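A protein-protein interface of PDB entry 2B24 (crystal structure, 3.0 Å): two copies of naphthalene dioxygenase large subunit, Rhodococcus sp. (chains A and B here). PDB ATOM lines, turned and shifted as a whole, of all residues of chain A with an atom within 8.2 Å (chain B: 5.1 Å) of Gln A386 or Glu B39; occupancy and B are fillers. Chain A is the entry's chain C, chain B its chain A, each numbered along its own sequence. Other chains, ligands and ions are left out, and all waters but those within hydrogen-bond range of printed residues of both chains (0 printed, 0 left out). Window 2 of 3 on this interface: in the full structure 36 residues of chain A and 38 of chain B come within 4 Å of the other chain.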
ATOM      1  N   GLU A   5      11.523 -25.958 -20.953  1.00  0.00           N
ATOM      2  CA  GLU A   5      11.779 -25.587 -19.562  1.00  0.00           C
ATOM      3  C   GLU A   5      10.510 -25.060 -18.865  1.00  0.00           C
ATOM      4  O   GLU A   5      10.236 -25.422 -17.718  1.00  0.00           O
ATOM      5  CB  GLU A   5      12.918 -24.562 -19.462  1.00  0.00           C
ATOM      6  CG  GLU A   5      14.294 -25.082 -19.846  1.00  0.00           C
ATOM      7  CD  GLU A   5      14.712 -24.665 -21.249  1.00  0.00           C
ATOM      8  OE1 GLU A   5      15.589 -23.778 -21.384  1.00  0.00           O
ATOM      9  OE2 GLU A   5      14.164 -25.230 -22.224  1.00  0.00           O
ATOM     10  N   ALA A  26       8.854 -18.525 -10.991  1.00  0.00           N
ATOM     11  CA  ALA A  26       9.150 -18.134 -12.373  1.00  0.00           C
ATOM     12  C   ALA A  26       7.933 -17.649 -13.137  1.00  0.00           C
ATOM     13  O   ALA A  26       8.041 -17.248 -14.288  1.00  0.00           O
ATOM     14  CB  ALA A  26       9.805 -19.298 -13.130  1.00  0.00           C
ATOM     15  N   ASN A  29       7.497 -12.845 -13.330  1.00  0.00           N
ATOM     16  CA  ASN A  29       8.175 -11.890 -14.204  1.00  0.00           C
ATOM     17  C   ASN A  29       9.022 -12.577 -15.281  1.00  0.00           C
ATOM     18  O   ASN A  29      10.254 -12.481 -15.279  1.00  0.00           O
ATOM     19  CB  ASN A  29       9.004 -10.905 -13.358  1.00  0.00           C
ATOM     20  CG  ASN A  29       9.345  -9.605 -14.099  1.00  0.00           C
ATOM     21  OD1 ASN A  29       9.477  -9.578 -15.317  1.00  0.00           O
ATOM     22  ND2 ASN A  29       9.519  -8.531 -13.351  1.00  0.00           N
ATOM     23  N   ASP A  30       8.363 -13.268 -16.210  1.00  0.00           N
ATOM     24  CA  ASP A  30       9.064 -13.918 -17.321  1.00  0.00           C
ATOM     25  C   ASP A  30       8.510 -13.410 -18.658  1.00  0.00           C
ATOM     26  O   ASP A  30       7.298 -13.353 -18.826  1.00  0.00           O
ATOM     27  CB  ASP A  30       8.914 -15.436 -17.223  1.00  0.00           C
ATOM     28  CG  ASP A  30      10.137 -16.201 -17.737  1.00  0.00           C
ATOM     29  OD1 ASP A  30      10.498 -16.068 -18.939  1.00  0.00           O
ATOM     30  OD2 ASP A  30      10.788 -16.994 -17.009  1.00  0.00           O
ATOM     31  N   VAL A 382      12.367  -7.905  -8.045  1.00  0.00           N
ATOM     32  CA  VAL A 382      13.306  -8.917  -7.577  1.00  0.00           C
ATOM     33  C   VAL A 382      13.019 -10.306  -8.160  1.00  0.00           C
ATOM     34  O   VAL A 382      13.937 -11.116  -8.312  1.00  0.00           O
ATOM     35  CB  VAL A 382      13.382  -8.933  -6.029  1.00  0.00           C
ATOM     36  CG1 VAL A 382      12.139  -9.545  -5.424  1.00  0.00           C
ATOM     37  CG2 VAL A 382      14.615  -9.666  -5.572  1.00  0.00           C
ATOM     38  N   MET A 383      11.754 -10.555  -8.504  1.00  0.00           N
ATOM     39  CA  MET A 383      11.332 -11.797  -9.144  1.00  0.00           C
ATOM     40  C   MET A 383      11.680 -11.808 -10.635  1.00  0.00           C
ATOM     41  O   MET A 383      11.092 -12.565 -11.416  1.00  0.00           O
ATOM     42  CB  MET A 383       9.823 -11.993  -8.972  1.00  0.00           C
ATOM     43  CG  MET A 383       9.379 -12.449  -7.584  1.00  0.00           C
ATOM     44  SD  MET A 383      10.140 -14.020  -7.065  1.00  0.00           S
ATOM     45  CE  MET A 383      11.445 -13.416  -5.997  1.00  0.00           C
ATOM     46  N   GLY A 384      12.630 -10.967 -11.033  1.00  0.00           N
ATOM     47  CA  GLY A 384      13.002 -10.838 -12.426  1.00  0.00           C
ATOM     48  C   GLY A 384      14.423 -11.279 -12.709  1.00  0.00           C
ATOM     49  O   GLY A 384      14.950 -11.026 -13.795  1.00  0.00           O
ATOM     50  N   GLY A 385      15.044 -11.934 -11.737  1.00  0.00           N
ATOM     51  CA  GLY A 385      16.389 -12.453 -11.909  1.00  0.00           C
ATOM     52  C   GLY A 385      16.324 -13.959 -11.923  1.00  0.00           C
ATOM     53  O   GLY A 385      15.324 -14.530 -11.484  1.00  0.00           O
ATOM     54  N   GLN A 386      17.387 -14.597 -12.403  1.00  0.00           N
ATOM     55  CA  GLN A 386      17.390 -16.048 -12.627  1.00  0.00           C
ATOM     56  C   GLN A 386      17.433 -16.887 -11.360  1.00  0.00           C
ATOM     57  O   GLN A 386      16.806 -17.940 -11.301  1.00  0.00           O
ATOM     58  CB  GLN A 386      18.527 -16.467 -13.561  1.00  0.00           C
ATOM     59  CG  GLN A 386      19.873 -15.926 -13.171  1.00  0.00           C
ATOM     60  CD  GLN A 386      20.942 -16.190 -14.202  1.00  0.00           C
ATOM     61  OE1 GLN A 386      20.681 -16.802 -15.233  1.00  0.00           O
ATOM     62  NE2 GLN A 386      22.159 -15.724 -13.927  1.00  0.00           N
ATOM     63  N   PHE A 387      18.174 -16.444 -10.354  1.00  0.00           N
ATOM     64  CA  PHE A 387      18.284 -17.223  -9.137  1.00  0.00           C
ATOM     65  C   PHE A 387      16.988 -17.140  -8.366  1.00  0.00           C
ATOM     66  O   PHE A 387      16.667 -18.051  -7.612  1.00  0.00           O
ATOM     67  CB  PHE A 387      19.455 -16.750  -8.273  1.00  0.00           C
ATOM     68  CG  PHE A 387      19.574 -17.472  -6.960  1.00  0.00           C
ATOM     69  CD1 PHE A 387      19.765 -18.845  -6.921  1.00  0.00           C
ATOM     70  CD2 PHE A 387      19.497 -16.784  -5.772  1.00  0.00           C
ATOM     71  CE1 PHE A 387      19.875 -19.511  -5.717  1.00  0.00           C
ATOM     72  CE2 PHE A 387      19.606 -17.447  -4.563  1.00  0.00           C
ATOM     73  CZ  PHE A 387      19.791 -18.813  -4.539  1.00  0.00           C
ATOM     74  N   ALA A 388      16.242 -16.054  -8.553  1.00  0.00           N
ATOM     75  CA  ALA A 388      14.983 -15.869  -7.845  1.00  0.00           C
ATOM     76  C   ALA A 388      13.870 -16.679  -8.483  1.00  0.00           C
ATOM     77  O   ALA A 388      13.026 -17.216  -7.778  1.00  0.00           O
ATOM     78  CB  ALA A 388      14.610 -14.399  -7.781  1.00  0.00           C
ATOM     79  N   LYS A 389      13.875 -16.768  -9.812  1.00  0.00           N
ATOM     80  CA  LYS A 389      12.848 -17.492 -10.564  1.00  0.00           C
ATOM     81  C   LYS A 389      12.969 -18.996 -10.351  1.00  0.00           C
ATOM     82  O   LYS A 389      12.085 -19.782 -10.727  1.00  0.00           O
ATOM     83  CB  LYS A 389      12.961 -17.178 -12.052  1.00  0.00           C
ATOM     84  CG  LYS A 389      12.129 -15.990 -12.476  1.00  0.00           C
ATOM     85  CD  LYS A 389      12.831 -15.226 -13.569  1.00  0.00           C
ATOM     86  CE  LYS A 389      12.153 -15.452 -14.878  1.00  0.00           C
ATOM     87  NZ  LYS A 389      12.901 -14.802 -15.968  1.00  0.00           N
ATOM     88  N   THR A 390      14.092 -19.368  -9.744  1.00  0.00           N
ATOM     89  CA  THR A 390      14.416 -20.721  -9.333  1.00  0.00           C
ATOM     90  C   THR A 390      13.624 -21.132  -8.092  1.00  0.00           C
ATOM     91  O   THR A 390      13.174 -22.272  -7.993  1.00  0.00           O
ATOM     92  CB  THR A 390      15.908 -20.752  -9.052  1.00  0.00           C
ATOM     93  OG1 THR A 390      16.619 -20.887 -10.291  1.00  0.00           O
ATOM     94  CG2 THR A 390      16.298 -21.967  -8.242  1.00  0.00           C
ATOM     95  N   GLY A 391      13.437 -20.193  -7.166  1.00  0.00           N
ATOM     96  CA  GLY A 391      12.680 -20.422  -5.943  1.00  0.00           C
ATOM     97  C   GLY A 391      11.193 -20.675  -6.101  1.00  0.00           C
ATOM     98  O   GLY A 391      10.733 -21.051  -7.180  1.00  0.00           O
ATOM     99  N   ASP B  35      21.506 -13.274 -23.203  1.00  0.00           N
ATOM    100  CA  ASP B  35      20.709 -14.226 -22.427  1.00  0.00           C
ATOM    101  C   ASP B  35      21.484 -15.513 -22.082  1.00  0.00           C
ATOM    102  O   ASP B  35      21.371 -16.037 -20.973  1.00  0.00           O
ATOM    103  CB  ASP B  35      19.398 -14.536 -23.149  1.00  0.00           C
ATOM    104  CG  ASP B  35      18.523 -13.316 -23.301  1.00  0.00           C
ATOM    105  OD1 ASP B  35      17.856 -13.168 -24.343  1.00  0.00           O
ATOM    106  OD2 ASP B  35      18.449 -12.439 -22.430  1.00  0.00           O
ATOM    107  N   VAL B  36      22.270 -16.003 -23.033  1.00  0.00           N
ATOM    108  CA  VAL B  36      23.146 -17.131 -22.809  1.00  0.00           C
ATOM    109  C   VAL B  36      24.201 -16.751 -21.771  1.00  0.00           C
ATOM    110  O   VAL B  36      24.548 -17.569 -20.912  1.00  0.00           O
ATOM    111  CB  VAL B  36      23.807 -17.592 -24.125  1.00  0.00           C
ATOM    112  CG1 VAL B  36      24.731 -18.758 -23.893  1.00  0.00           C
ATOM    113  CG2 VAL B  36      22.750 -17.995 -25.130  1.00  0.00           C
ATOM    114  N   GLU B  37      24.691 -15.510 -21.849  1.00  0.00           N
ATOM    115  CA  GLU B  37      25.710 -14.989 -20.942  1.00  0.00           C
ATOM    116  C   GLU B  37      25.205 -14.872 -19.513  1.00  0.00           C
ATOM    117  O   GLU B  37      25.985 -14.905 -18.569  1.00  0.00           O
ATOM    118  CB  GLU B  37      26.191 -13.633 -21.430  1.00  0.00           C
ATOM    119  CG  GLU B  37      27.447 -13.113 -20.766  1.00  0.00           C
ATOM    120  CD  GLU B  37      27.890 -11.786 -21.339  1.00  0.00           C
ATOM    121  OE1 GLU B  37      27.246 -10.756 -21.011  1.00  0.00           O
ATOM    122  OE2 GLU B  37      28.877 -11.771 -22.107  1.00  0.00           O
ATOM    123  N   ARG B  38      23.894 -14.735 -19.359  1.00  0.00           N
ATOM    124  CA  ARG B  38      23.278 -14.628 -18.046  1.00  0.00           C
ATOM    125  C   ARG B  38      23.498 -15.913 -17.263  1.00  0.00           C
ATOM    126  O   ARG B  38      23.958 -15.867 -16.132  1.00  0.00           O
ATOM    127  CB  ARG B  38      21.791 -14.330 -18.191  1.00  0.00           C
ATOM    128  CG  ARG B  38      21.151 -13.693 -16.993  1.00  0.00           C
ATOM    129  CD  ARG B  38      19.692 -13.380 -17.192  1.00  0.00           C
ATOM    130  NE  ARG B  38      19.510 -11.973 -17.490  1.00  0.00           N
ATOM    131  CZ  ARG B  38      19.036 -11.489 -18.630  1.00  0.00           C
ATOM    132  NH1 ARG B  38      18.683 -12.300 -19.615  1.00  0.00           N
ATOM    133  NH2 ARG B  38      18.924 -10.175 -18.791  1.00  0.00           N
ATOM    134  N   GLU B  39      23.182 -17.059 -17.866  1.00  0.00           N
ATOM    135  CA  GLU B  39      23.439 -18.345 -17.233  1.00  0.00           C
ATOM    136  C   GLU B  39      24.914 -18.740 -17.335  1.00  0.00           C
ATOM    137  O   GLU B  39      25.545 -19.003 -16.316  1.00  0.00           O
ATOM    138  CB  GLU B  39      22.546 -19.454 -17.804  1.00  0.00           C
ATOM    139  CG  GLU B  39      22.315 -20.598 -16.817  1.00  0.00           C
ATOM    140  CD  GLU B  39      22.640 -21.996 -17.353  1.00  0.00           C
ATOM    141  OE1 GLU B  39      23.558 -22.152 -18.202  1.00  0.00           O
ATOM    142  OE2 GLU B  39      21.972 -22.958 -16.890  1.00  0.00           O
ATOM    143  N   ARG B  40      25.466 -18.767 -18.545  1.00  0.00           N
ATOM    144  CA  ARG B  40      26.787 -19.348 -18.756  1.00  0.00           C
ATOM    145  C   ARG B  40      27.947 -18.655 -18.030  1.00  0.00           C
ATOM    146  O   ARG B  40      28.824 -19.332 -17.486  1.00  0.00           O
ATOM    147  CB  ARG B  40      27.103 -19.474 -20.249  1.00  0.00           C
ATOM    148  CG  ARG B  40      26.271 -20.488 -21.036  1.00  0.00           C
ATOM    149  CD  ARG B  40      26.526 -21.961 -20.729  1.00  0.00           C
ATOM    150  NE  ARG B  40      25.253 -22.688 -20.619  1.00  0.00           N
ATOM    151  CZ  ARG B  40      24.504 -23.080 -21.655  1.00  0.00           C
ATOM    152  NH1 ARG B  40      24.906 -22.839 -22.900  1.00  0.00           N
ATOM    153  NH2 ARG B  40      23.356 -23.721 -21.447  1.00  0.00           N
ATOM    154  N   ILE B  41      27.957 -17.326 -18.027  1.00  0.00           N
ATOM    155  CA  ILE B  41      29.006 -16.535 -17.367  1.00  0.00           C
ATOM    156  C   ILE B  41      28.617 -16.084 -15.950  1.00  0.00           C
ATOM    157  O   ILE B  41      29.288 -16.427 -14.978  1.00  0.00           O
ATOM    158  CB  ILE B  41      29.348 -15.284 -18.195  1.00  0.00           C
ATOM    159  CG1 ILE B  41      29.632 -15.641 -19.655  1.00  0.00           C
ATOM    160  CG2 ILE B  41      30.480 -14.518 -17.564  1.00  0.00           C
ATOM    161  CD1 ILE B  41      30.773 -16.589 -19.914  1.00  0.00           C
ATOM    162  N   PHE B  42      27.538 -15.306 -15.843  1.00  0.00           N
ATOM    163  CA  PHE B  42      27.141 -14.720 -14.571  1.00  0.00           C
ATOM    164  C   PHE B  42      26.412 -15.695 -13.671  1.00  0.00           C
ATOM    165  O   PHE B  42      26.248 -15.422 -12.486  1.00  0.00           O
ATOM    166  CB  PHE B  42      26.328 -13.443 -14.798  1.00  0.00           C
ATOM    167  CG  PHE B  42      27.136 -12.332 -15.383  1.00  0.00           C
ATOM    168  CD1 PHE B  42      27.087 -12.055 -16.729  1.00  0.00           C
ATOM    169  CD2 PHE B  42      27.996 -11.590 -14.593  1.00  0.00           C
ATOM    170  CE1 PHE B  42      27.858 -11.046 -17.272  1.00  0.00           C
ATOM    171  CE2 PHE B  42      28.763 -10.585 -15.138  1.00  0.00           C
ATOM    172  CZ  PHE B  42      28.693 -10.322 -16.476  1.00  0.00           C
ATOM    173  N   GLY B  43      25.991 -16.829 -14.232  1.00  0.00           N
ATOM    174  CA  GLY B  43      25.256 -17.831 -13.486  1.00  0.00           C
ATOM    175  C   GLY B  43      26.155 -18.885 -12.885  1.00  0.00           C
ATOM    176  O   GLY B  43      25.681 -19.785 -12.183  1.00  0.00           O
ATOM    177  N   HIS B  44      27.453 -18.756 -13.159  1.00  0.00           N
ATOM    178  CA  HIS B  44      28.465 -19.684 -12.666  1.00  0.00           C
ATOM    179  C   HIS B  44      29.702 -18.993 -12.089  1.00  0.00           C
ATOM    180  O   HIS B  44      30.094 -19.296 -10.969  1.00  0.00           O
ATOM    181  CB  HIS B  44      28.855 -20.659 -13.775  1.00  0.00           C
ATOM    182  CG  HIS B  44      27.722 -21.519 -14.230  1.00  0.00           C
ATOM    183  ND1 HIS B  44      26.976 -22.282 -13.357  1.00  0.00           N
ATOM    184  CD2 HIS B  44      27.194 -21.724 -15.459  1.00  0.00           C
ATOM    185  CE1 HIS B  44      26.041 -22.929 -14.030  1.00  0.00           C
ATOM    186  NE2 HIS B  44      26.149 -22.604 -15.307  1.00  0.00           N
ATOM    187  N   SER B  67      23.953 -10.045 -11.860  1.00  0.00           N
ATOM    188  CA  SER B  67      23.003  -9.674 -12.909  1.00  0.00           C
ATOM    189  C   SER B  67      21.736  -9.076 -12.305  1.00  0.00           C
ATOM    190  O   SER B  67      21.813  -8.127 -11.537  1.00  0.00           O
ATOM    191  CB  SER B  67      22.681 -10.866 -13.796  1.00  0.00           C
ATOM    192  OG  SER B  67      23.322 -10.707 -15.039  1.00  0.00           O
ATOM    193  N   ASP B  69      19.709 -10.393 -10.123  1.00  0.00           N
ATOM    194  CA  ASP B  69      19.440 -10.911  -8.776  1.00  0.00           C
ATOM    195  C   ASP B  69      19.938  -9.965  -7.691  1.00  0.00           C
ATOM    196  O   ASP B  69      21.120  -9.606  -7.644  1.00  0.00           O
ATOM    197  CB  ASP B  69      20.064 -12.294  -8.569  1.00  0.00           C
ATOM    198  CG  ASP B  69      19.454 -13.339  -9.448  1.00  0.00           C
ATOM    199  OD1 ASP B  69      18.330 -13.805  -9.148  1.00  0.00           O
ATOM    200  OD2 ASP B  69      20.025 -13.748 -10.478  1.00  0.00           O
ATOM    201  N   LEU B 159      26.508 -18.156  -8.127  1.00  0.00           N
ATOM    202  CA  LEU B 159      25.164 -18.729  -8.180  1.00  0.00           C
ATOM    203  C   LEU B 159      25.190 -20.251  -8.315  1.00  0.00           C
ATOM    204  O   LEU B 159      24.161 -20.908  -8.170  1.00  0.00           O
ATOM    205  CB  LEU B 159      24.394 -18.115  -9.353  1.00  0.00           C
ATOM    206  CG  LEU B 159      23.212 -17.186  -9.098  1.00  0.00           C
ATOM    207  CD1 LEU B 159      23.425 -16.322  -7.888  1.00  0.00           C
ATOM    208  CD2 LEU B 159      22.999 -16.340 -10.317  1.00  0.00           C
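Glu A5 touches none of the printed residues of chain B. Of the printed residues of chain B, Gly A385 touches Asp B69. Of the printed residues of chain B, Phe A387 touches Asp B69 and Leu B159. Of chain A, only Gln A386 (3.6 Å) comes within 4 Å of Glu B39. Printed residues of chain A within 4 Å of Asp B69: Gly A385 (3.4 Å), Gln A386 (3.4 Å), Phe A387 (2.9 Å) and Ala A388 (3.1 Å). The nearest residue of chain B that does not touch Gln A386 is Phe B42 (4.3 Å). The nearest printed residue of chain B that does not touch Ala A388 is Leu B159 (7.0 Å).
No position is printed for both chains. Of the 9 pairs that touch across the chains among the printed residues, none has its exchanged pair printed and touching as well.
Among the printed residues, merely in contact across the chains: Gly A385 with Asp B69, Gln A386 with Glu B39, Gln A386 with Leu B159, Gln A386 with Gly B43 and Phe A387 with Leu B159.
The side-chain amide nitrogen (NE2) of Gln A386 sits at hydrogen-bond distance from the backbone carbonyl oxygen (O) of Arg B38, 2.8 Å away. OD2 of Asp B69 is in hydrogen-bond range of N of Gln A386 (3.4 Å). OD1 of Asp B69 is in hydrogen-bond range of N of Phe A387, at 2.9 Å. The side-chain carboxylate (OD1) of Asp B69 sits at hydrogen-bond distance from the backbone NH (N) of Ala A388 (3.1 Å).
The guanidinium group (NH1) of Arg B38 lies within salt-bridge range of the side-chain carboxylate (OD2) of Asp B35 (2.8 Å). O of Arg B38 is in hydrogen-bond range of N of Gly B43 (2.9 Å). The side-chain carboxylate (OE1) of Glu B39 lies within salt-bridge range of the guanidinium group (NE) of Arg B40, 3.0 Å away. The backbone carbonyl oxygen (O) of Gln A386 sits at hydrogen-bond distance from the side-chain hydroxyl (OG1) of Thr A390, at 3.1 Å.
Hydrophobic or aromatic side chains of chain B within 4 Å of the printed part of chain A: Leu B159. Of the 14 printed residues of chain A, 4 touch a printed residue of chain B. Among the printed residues, no Asp or Glu carboxylate lies within 4 Å of a Lys or Arg side-chain nitrogen of the other chain.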
